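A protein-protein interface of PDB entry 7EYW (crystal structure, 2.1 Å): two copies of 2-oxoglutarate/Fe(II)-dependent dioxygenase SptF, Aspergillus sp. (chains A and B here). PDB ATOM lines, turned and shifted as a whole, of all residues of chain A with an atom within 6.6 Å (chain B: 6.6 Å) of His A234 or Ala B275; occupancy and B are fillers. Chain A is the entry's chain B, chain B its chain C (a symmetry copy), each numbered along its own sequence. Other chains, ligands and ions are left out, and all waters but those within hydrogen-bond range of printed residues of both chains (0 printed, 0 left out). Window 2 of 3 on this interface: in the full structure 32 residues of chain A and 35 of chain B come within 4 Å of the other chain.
Hydrophobic or aromatic side chains of chain B that line the printed part of chain A: Ala B267 and Ala B275. Hydrophobic or aromatic side chains of chain A within 4 Å of the printed part of chain B: His A234. Among the printed residues, 7 pairs touch across the chains. Among the printed residues, no Asp or Glu carboxylate lies within 4 Å of a Lys or Arg side-chain nitrogen of the other chain.
Of the printed residues of chain B, Asn A73 touches Ala B267 and Gly B268. Of the printed residues of chain B, His A234 touches Ala B267, Ala B275 and Thr B276. Pro A236 touches none of the printed residues of chain B. Of the printed residues of chain A, Lys B266 touches Ser A231 (2.5 Å). Ala B275 touches just one residue of chain A: His A234 (3.5 Å). The nearest residue of chain A that does not touch Ala B275 is Ser A72 (6.0 Å).
The backbone NH of Gly B268 lies within hydrogen-bond range of the side-chain amide oxygen of Asn A73 (2.6 Å). The backbone NH of Ser A231 sits at hydrogen-bond distance from the backbone carbonyl oxygen of Lys B266 (2.5 Å).
Among the printed residues, merely in contact across the chains: Asn A73 with Ala B267, His A234 with Ala B275, Ser A72 with Gly B268, His A234 with Thr B276 and His A234 with Ala B267.
The side-chain amide oxygen (OD1) of Asn A73 lies within hydrogen-bond range of the side-chain hydroxyl (OG) of Ser A72, 3.0 Å away. The side-chain amide nitrogen (ND2) of Asn A73 is in hydrogen-bond range of the backbone carbonyl oxygen (O) of Ser A231. ND2 of Asn A73 is in hydrogen-bond range of NE2 of His A232. A ring nitrogen (NE2) of His A234 lies within hydrogen-bond range of the side-chain amide oxygen of Asn A73, at 2.9 Å. OG1 of Thr B276 is in hydrogen-bond range of O of Leu B272 (2.8 Å). O of Glu B273 sits close to OG1 of Thr B276, at 3.4 Å.
No position is printed for both chains. Of the 7 pairs that touch across the chains among the printed residues, none has its exchanged pair printed and touching as well.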
ATOM      1  N   SER A  72      17.744  -8.788  17.557  1.00  0.00           N
ATOM      2  CA  SER A  72      17.128 -10.057  17.180  1.00  0.00           C
ATOM      3  C   SER A  72      17.840 -11.227  17.851  1.00  0.00           C
ATOM      4  O   SER A  72      18.318 -11.100  18.981  1.00  0.00           O
ATOM      5  CB  SER A  72      17.127 -10.247  15.664  1.00  0.00           C
ATOM      6  OG  SER A  72      16.487 -11.455  15.304  1.00  0.00           O
ATOM      7  N   ASN A  73      17.899 -12.375  17.178  1.00  0.00           N
ATOM      8  CA  ASN A  73      18.585 -13.529  17.746  1.00  0.00           C
ATOM      9  C   ASN A  73      20.077 -13.248  17.867  1.00  0.00           C
ATOM     10  O   ASN A  73      20.679 -12.607  16.999  1.00  0.00           O
ATOM     11  CB  ASN A  73      18.342 -14.780  16.896  1.00  0.00           C
ATOM     12  CG  ASN A  73      16.871 -15.104  16.752  1.00  0.00           C
ATOM     13  OD1 ASN A  73      16.090 -14.283  16.272  1.00  0.00           O
ATOM     14  ND2 ASN A  73      16.485 -16.303  17.165  1.00  0.00           N
ATOM     15  N   LEU A  76      21.994 -14.436  15.052  1.00  0.00           N
ATOM     16  CA  LEU A  76      21.881 -13.569  13.885  1.00  0.00           C
ATOM     17  C   LEU A  76      22.757 -12.332  14.028  1.00  0.00           C
ATOM     18  O   LEU A  76      23.378 -11.889  13.054  1.00  0.00           O
ATOM     19  CB  LEU A  76      20.420 -13.165  13.674  1.00  0.00           C
ATOM     20  CG  LEU A  76      20.109 -12.072  12.644  1.00  0.00           C
ATOM     21  CD1 LEU A  76      20.631 -12.435  11.262  1.00  0.00           C
ATOM     22  CD2 LEU A  76      18.616 -11.783  12.601  1.00  0.00           C
ATOM     23  N   SER A 231      13.173 -19.244  17.232  1.00  0.00           N
ATOM     24  CA  SER A 231      13.378 -19.845  15.925  1.00  0.00           C
ATOM     25  C   SER A 231      14.475 -19.082  15.195  1.00  0.00           C
ATOM     26  O   SER A 231      14.681 -17.888  15.425  1.00  0.00           O
ATOM     27  CB  SER A 231      12.087 -19.832  15.102  1.00  0.00           C
ATOM     28  OG  SER A 231      12.264 -20.500  13.864  1.00  0.00           O
ATOM     29  N   HIS A 232      15.188 -19.783  14.313  1.00  0.00           N
ATOM     30  CA  HIS A 232      16.303 -19.191  13.583  1.00  0.00           C
ATOM     31  C   HIS A 232      16.151 -19.345  12.074  1.00  0.00           C
ATOM     32  O   HIS A 232      17.136 -19.234  11.339  1.00  0.00           O
ATOM     33  CB  HIS A 232      17.628 -19.799  14.048  1.00  0.00           C
ATOM     34  CG  HIS A 232      17.978 -19.475  15.468  1.00  0.00           C
ATOM     35  ND1 HIS A 232      17.490 -20.196  16.536  1.00  0.00           N
ATOM     36  CD2 HIS A 232      18.767 -18.510  15.994  1.00  0.00           C
ATOM     37  CE1 HIS A 232      17.964 -19.688  17.660  1.00  0.00           C
ATOM     38  NE2 HIS A 232      18.743 -18.665  17.359  1.00  0.00           N
ATOM     39  N   HIS A 233      14.935 -19.581  11.595  1.00  0.00           N
ATOM     40  CA  HIS A 233      14.694 -19.823  10.181  1.00  0.00           C
ATOM     41  C   HIS A 233      14.438 -18.543   9.397  1.00  0.00           C
ATOM     42  O   HIS A 233      14.217 -18.608   8.184  1.00  0.00           O
ATOM     43  CB  HIS A 233      13.530 -20.802  10.035  1.00  0.00           C
ATOM     44  CG  HIS A 233      13.812 -22.147  10.630  1.00  0.00           C
ATOM     45  ND1 HIS A 233      12.837 -23.102  10.812  1.00  0.00           N
ATOM     46  CD2 HIS A 233      14.967 -22.702  11.069  1.00  0.00           C
ATOM     47  CE1 HIS A 233      13.375 -24.183  11.347  1.00  0.00           C
ATOM     48  NE2 HIS A 233      14.667 -23.965  11.515  1.00  0.00           N
ATOM     49  N   HIS A 234      14.463 -17.389  10.062  1.00  0.00           N
ATOM     50  CA  HIS A 234      14.532 -16.102   9.385  1.00  0.00           C
ATOM     51  C   HIS A 234      15.961 -15.700   9.052  1.00  0.00           C
ATOM     52  O   HIS A 234      16.169 -14.647   8.442  1.00  0.00           O
ATOM     53  CB  HIS A 234      13.874 -15.014  10.242  1.00  0.00           C
ATOM     54  CG  HIS A 234      14.524 -14.819  11.578  1.00  0.00           C
ATOM     55  ND1 HIS A 234      14.718 -15.851  12.470  1.00  0.00           N
ATOM     56  CD2 HIS A 234      15.027 -13.710  12.171  1.00  0.00           C
ATOM     57  CE1 HIS A 234      15.310 -15.389  13.556  1.00  0.00           C
ATOM     58  NE2 HIS A 234      15.509 -14.091  13.401  1.00  0.00           N
ATOM     59  N   LEU A 235      16.946 -16.515   9.439  1.00  0.00           N
ATOM     60  CA  LEU A 235      18.350 -16.236   9.177  1.00  0.00           C
ATOM     61  C   LEU A 235      18.686 -16.553   7.720  1.00  0.00           C
ATOM     62  O   LEU A 235      18.160 -17.518   7.158  1.00  0.00           O
ATOM     63  CB  LEU A 235      19.242 -17.061  10.103  1.00  0.00           C
ATOM     64  CG  LEU A 235      19.729 -16.391  11.391  1.00  0.00           C
ATOM     65  CD1 LEU A 235      18.579 -16.195  12.364  1.00  0.00           C
ATOM     66  CD2 LEU A 235      20.843 -17.207  12.031  1.00  0.00           C
ATOM     67  N   PRO A 236      19.549 -15.760   7.091  1.00  0.00           N
ATOM     68  CA  PRO A 236      19.930 -16.035   5.701  1.00  0.00           C
ATOM     69  C   PRO A 236      20.681 -17.351   5.576  1.00  0.00           C
ATOM     70  O   PRO A 236      21.274 -17.860   6.530  1.00  0.00           O
ATOM     71  CB  PRO A 236      20.823 -14.846   5.329  1.00  0.00           C
ATOM     72  CG  PRO A 236      21.292 -14.287   6.631  1.00  0.00           C
ATOM     73  CD  PRO A 236      20.190 -14.542   7.615  1.00  0.00           C
ATOM     74  N   PHE A 253      18.184 -26.567  12.009  1.00  0.00           N
ATOM     75  CA  PHE A 253      18.311 -26.803  10.577  1.00  0.00           C
ATOM     76  C   PHE A 253      18.582 -28.259  10.233  1.00  0.00           C
ATOM     77  O   PHE A 253      18.758 -28.580   9.053  1.00  0.00           O
ATOM     78  CB  PHE A 253      19.420 -25.921   9.994  1.00  0.00           C
ATOM     79  CG  PHE A 253      19.170 -24.454  10.162  1.00  0.00           C
ATOM     80  CD1 PHE A 253      18.258 -23.796   9.354  1.00  0.00           C
ATOM     81  CD2 PHE A 253      19.836 -23.734  11.139  1.00  0.00           C
ATOM     82  CE1 PHE A 253      18.021 -22.445   9.512  1.00  0.00           C
ATOM     83  CE2 PHE A 253      19.604 -22.383  11.303  1.00  0.00           C
ATOM     84  CZ  PHE A 253      18.695 -21.739  10.489  1.00  0.00           C
ATOM     85  N   LYS B 266      10.127 -17.848  18.675  1.00  0.00           N
ATOM     86  CA  LYS B 266      10.208 -16.417  18.424  1.00  0.00           C
ATOM     87  C   LYS B 266      11.333 -16.094  17.449  1.00  0.00           C
ATOM     88  O   LYS B 266      12.235 -16.899  17.202  1.00  0.00           O
ATOM     89  CB  LYS B 266      10.442 -15.650  19.726  1.00  0.00           C
ATOM     90  CG  LYS B 266       9.257 -15.598  20.672  1.00  0.00           C
ATOM     91  CD  LYS B 266       9.729 -15.497  22.118  1.00  0.00           C
ATOM     92  CE  LYS B 266      10.967 -14.621  22.241  1.00  0.00           C
ATOM     93  NZ  LYS B 266      11.494 -14.568  23.631  1.00  0.00           N
ATOM     94  N   ALA B 267      11.272 -14.884  16.903  1.00  0.00           N
ATOM     95  CA  ALA B 267      12.343 -14.307  16.096  1.00  0.00           C
ATOM     96  C   ALA B 267      12.991 -13.220  16.949  1.00  0.00           C
ATOM     97  O   ALA B 267      12.595 -12.053  16.902  1.00  0.00           O
ATOM     98  CB  ALA B 267      11.809 -13.754  14.779  1.00  0.00           C
ATOM     99  N   GLY B 268      13.988 -13.614  17.738  1.00  0.00           N
ATOM    100  CA  GLY B 268      14.610 -12.703  18.679  1.00  0.00           C
ATOM    101  C   GLY B 268      13.655 -12.294  19.779  1.00  0.00           C
ATOM    102  O   GLY B 268      13.415 -13.057  20.720  1.00  0.00           O
ATOM    103  N   GLY B 270      10.671 -10.423  18.588  1.00  0.00           N
ATOM    104  CA  GLY B 270       9.430 -10.296  17.860  1.00  0.00           C
ATOM    105  C   GLY B 270       8.920 -11.634  17.356  1.00  0.00           C
ATOM    106  O   GLY B 270       9.380 -12.707  17.754  1.00  0.00           O
ATOM    107  N   ASN B 271       7.950 -11.558  16.452  1.00  0.00           N
ATOM    108  CA  ASN B 271       7.329 -12.747  15.891  1.00  0.00           C
ATOM    109  C   ASN B 271       8.103 -13.237  14.674  1.00  0.00           C
ATOM    110  O   ASN B 271       8.712 -12.454  13.941  1.00  0.00           O
ATOM    111  CB  ASN B 271       5.876 -12.465  15.507  1.00  0.00           C
ATOM    112  CG  ASN B 271       5.010 -12.138  16.706  1.00  0.00           C
ATOM    113  OD1 ASN B 271       5.294 -12.565  17.825  1.00  0.00           O
ATOM    114  ND2 ASN B 271       3.945 -11.378  16.479  1.00  0.00           N
ATOM    115  N   LEU B 272       8.074 -14.557  14.470  1.00  0.00           N
ATOM    116  CA  LEU B 272       8.739 -15.143  13.311  1.00  0.00           C
ATOM    117  C   LEU B 272       8.119 -14.647  12.011  1.00  0.00           C
ATOM    118  O   LEU B 272       8.828 -14.414  11.025  1.00  0.00           O
ATOM    119  CB  LEU B 272       8.674 -16.670  13.387  1.00  0.00           C
ATOM    120  CG  LEU B 272       9.195 -17.456  12.181  1.00  0.00           C
ATOM    121  CD1 LEU B 272      10.695 -17.254  12.003  1.00  0.00           C
ATOM    122  CD2 LEU B 272       8.855 -18.934  12.318  1.00  0.00           C
ATOM    123  N   GLU B 273       6.796 -14.473  11.992  1.00  0.00           N
ATOM    124  CA  GLU B 273       6.123 -13.991  10.793  1.00  0.00           C
ATOM    125  C   GLU B 273       6.482 -12.546  10.467  1.00  0.00           C
ATOM    126  O   GLU B 273       6.370 -12.141   9.306  1.00  0.00           O
ATOM    127  CB  GLU B 273       4.607 -14.135  10.946  1.00  0.00           C
ATOM    128  CG  GLU B 273       4.032 -13.439  12.167  1.00  0.00           C
ATOM    129  CD  GLU B 273       3.840 -14.384  13.337  1.00  0.00           C
ATOM    130  OE1 GLU B 273       4.777 -15.150  13.646  1.00  0.00           O
ATOM    131  OE2 GLU B 273       2.749 -14.365  13.946  1.00  0.00           O
ATOM    132  N   ASP B 274       6.908 -11.763  11.461  1.00  0.00           N
ATOM    133  CA  ASP B 274       7.383 -10.412  11.182  1.00  0.00           C
ATOM    134  C   ASP B 274       8.765 -10.443  10.544  1.00  0.00           C
ATOM    135  O   ASP B 274       9.022  -9.743   9.557  1.00  0.00           O
ATOM    136  CB  ASP B 274       7.406  -9.582  12.466  1.00  0.00           C
ATOM    137  CG  ASP B 274       6.021  -9.318  13.017  1.00  0.00           C
ATOM    138  OD1 ASP B 274       5.052  -9.333  12.229  1.00  0.00           O
ATOM    139  OD2 ASP B 274       5.902  -9.093  14.240  1.00  0.00           O
ATOM    140  N   ALA B 275       9.671 -11.255  11.095  1.00  0.00           N
ATOM    141  CA  ALA B 275      11.025 -11.329  10.562  1.00  0.00           C
ATOM    142  C   ALA B 275      11.054 -11.929   9.162  1.00  0.00           C
ATOM    143  O   ALA B 275      11.976 -11.647   8.388  1.00  0.00           O
ATOM    144  CB  ALA B 275      11.916 -12.137  11.505  1.00  0.00           C
ATOM    145  N   THR B 276      10.065 -12.755   8.820  1.00  0.00           N
ATOM    146  CA  THR B 276       9.981 -13.353   7.494  1.00  0.00           C
ATOM    147  C   THR B 276       9.076 -12.576   6.545  1.00  0.00           C
ATOM    148  O   THR B 276       9.011 -12.920   5.360  1.00  0.00           O
ATOM    149  CB  THR B 276       9.487 -14.801   7.590  1.00  0.00           C
ATOM    150  OG1 THR B 276       8.273 -14.848   8.350  1.00  0.00           O
ATOM    151  CG2 THR B 276      10.536 -15.677   8.259  1.00  0.00           C
ATOM    152  N   GLY B 277       8.382 -11.549   7.031  1.00  0.00           N
ATOM    153  CA  GLY B 277       7.549 -10.720   6.183  1.00  0.00           C
ATOM    154  C   GLY B 277       6.399 -11.457   5.532  1.00  0.00           C
ATOM    155  O   GLY B 277       6.226 -11.394   4.311  1.00  0.00           O
ATOM    156  N   LEU B 278       5.601 -12.154   6.333  1.00  0.00           N
ATOM    157  CA  LEU B 278       4.467 -12.909   5.813  1.00  0.00           C
ATOM    158  C   LEU B 278       3.287 -11.989   5.514  1.00  0.00           C
ATOM    159  O   LEU B 278       2.618 -11.504   6.426  1.00  0.00           O
ATOM    160  CB  LEU B 278       4.051 -14.000   6.800  1.00  0.00           C
ATOM    161  CG  LEU B 278       4.848 -15.305   6.745  1.00  0.00           C
ATOM    162  CD1 LEU B 278       4.155 -16.391   7.553  1.00  0.00           C
ATOM    163  CD2 LEU B 278       5.048 -15.752   5.306  1.00  0.00           C
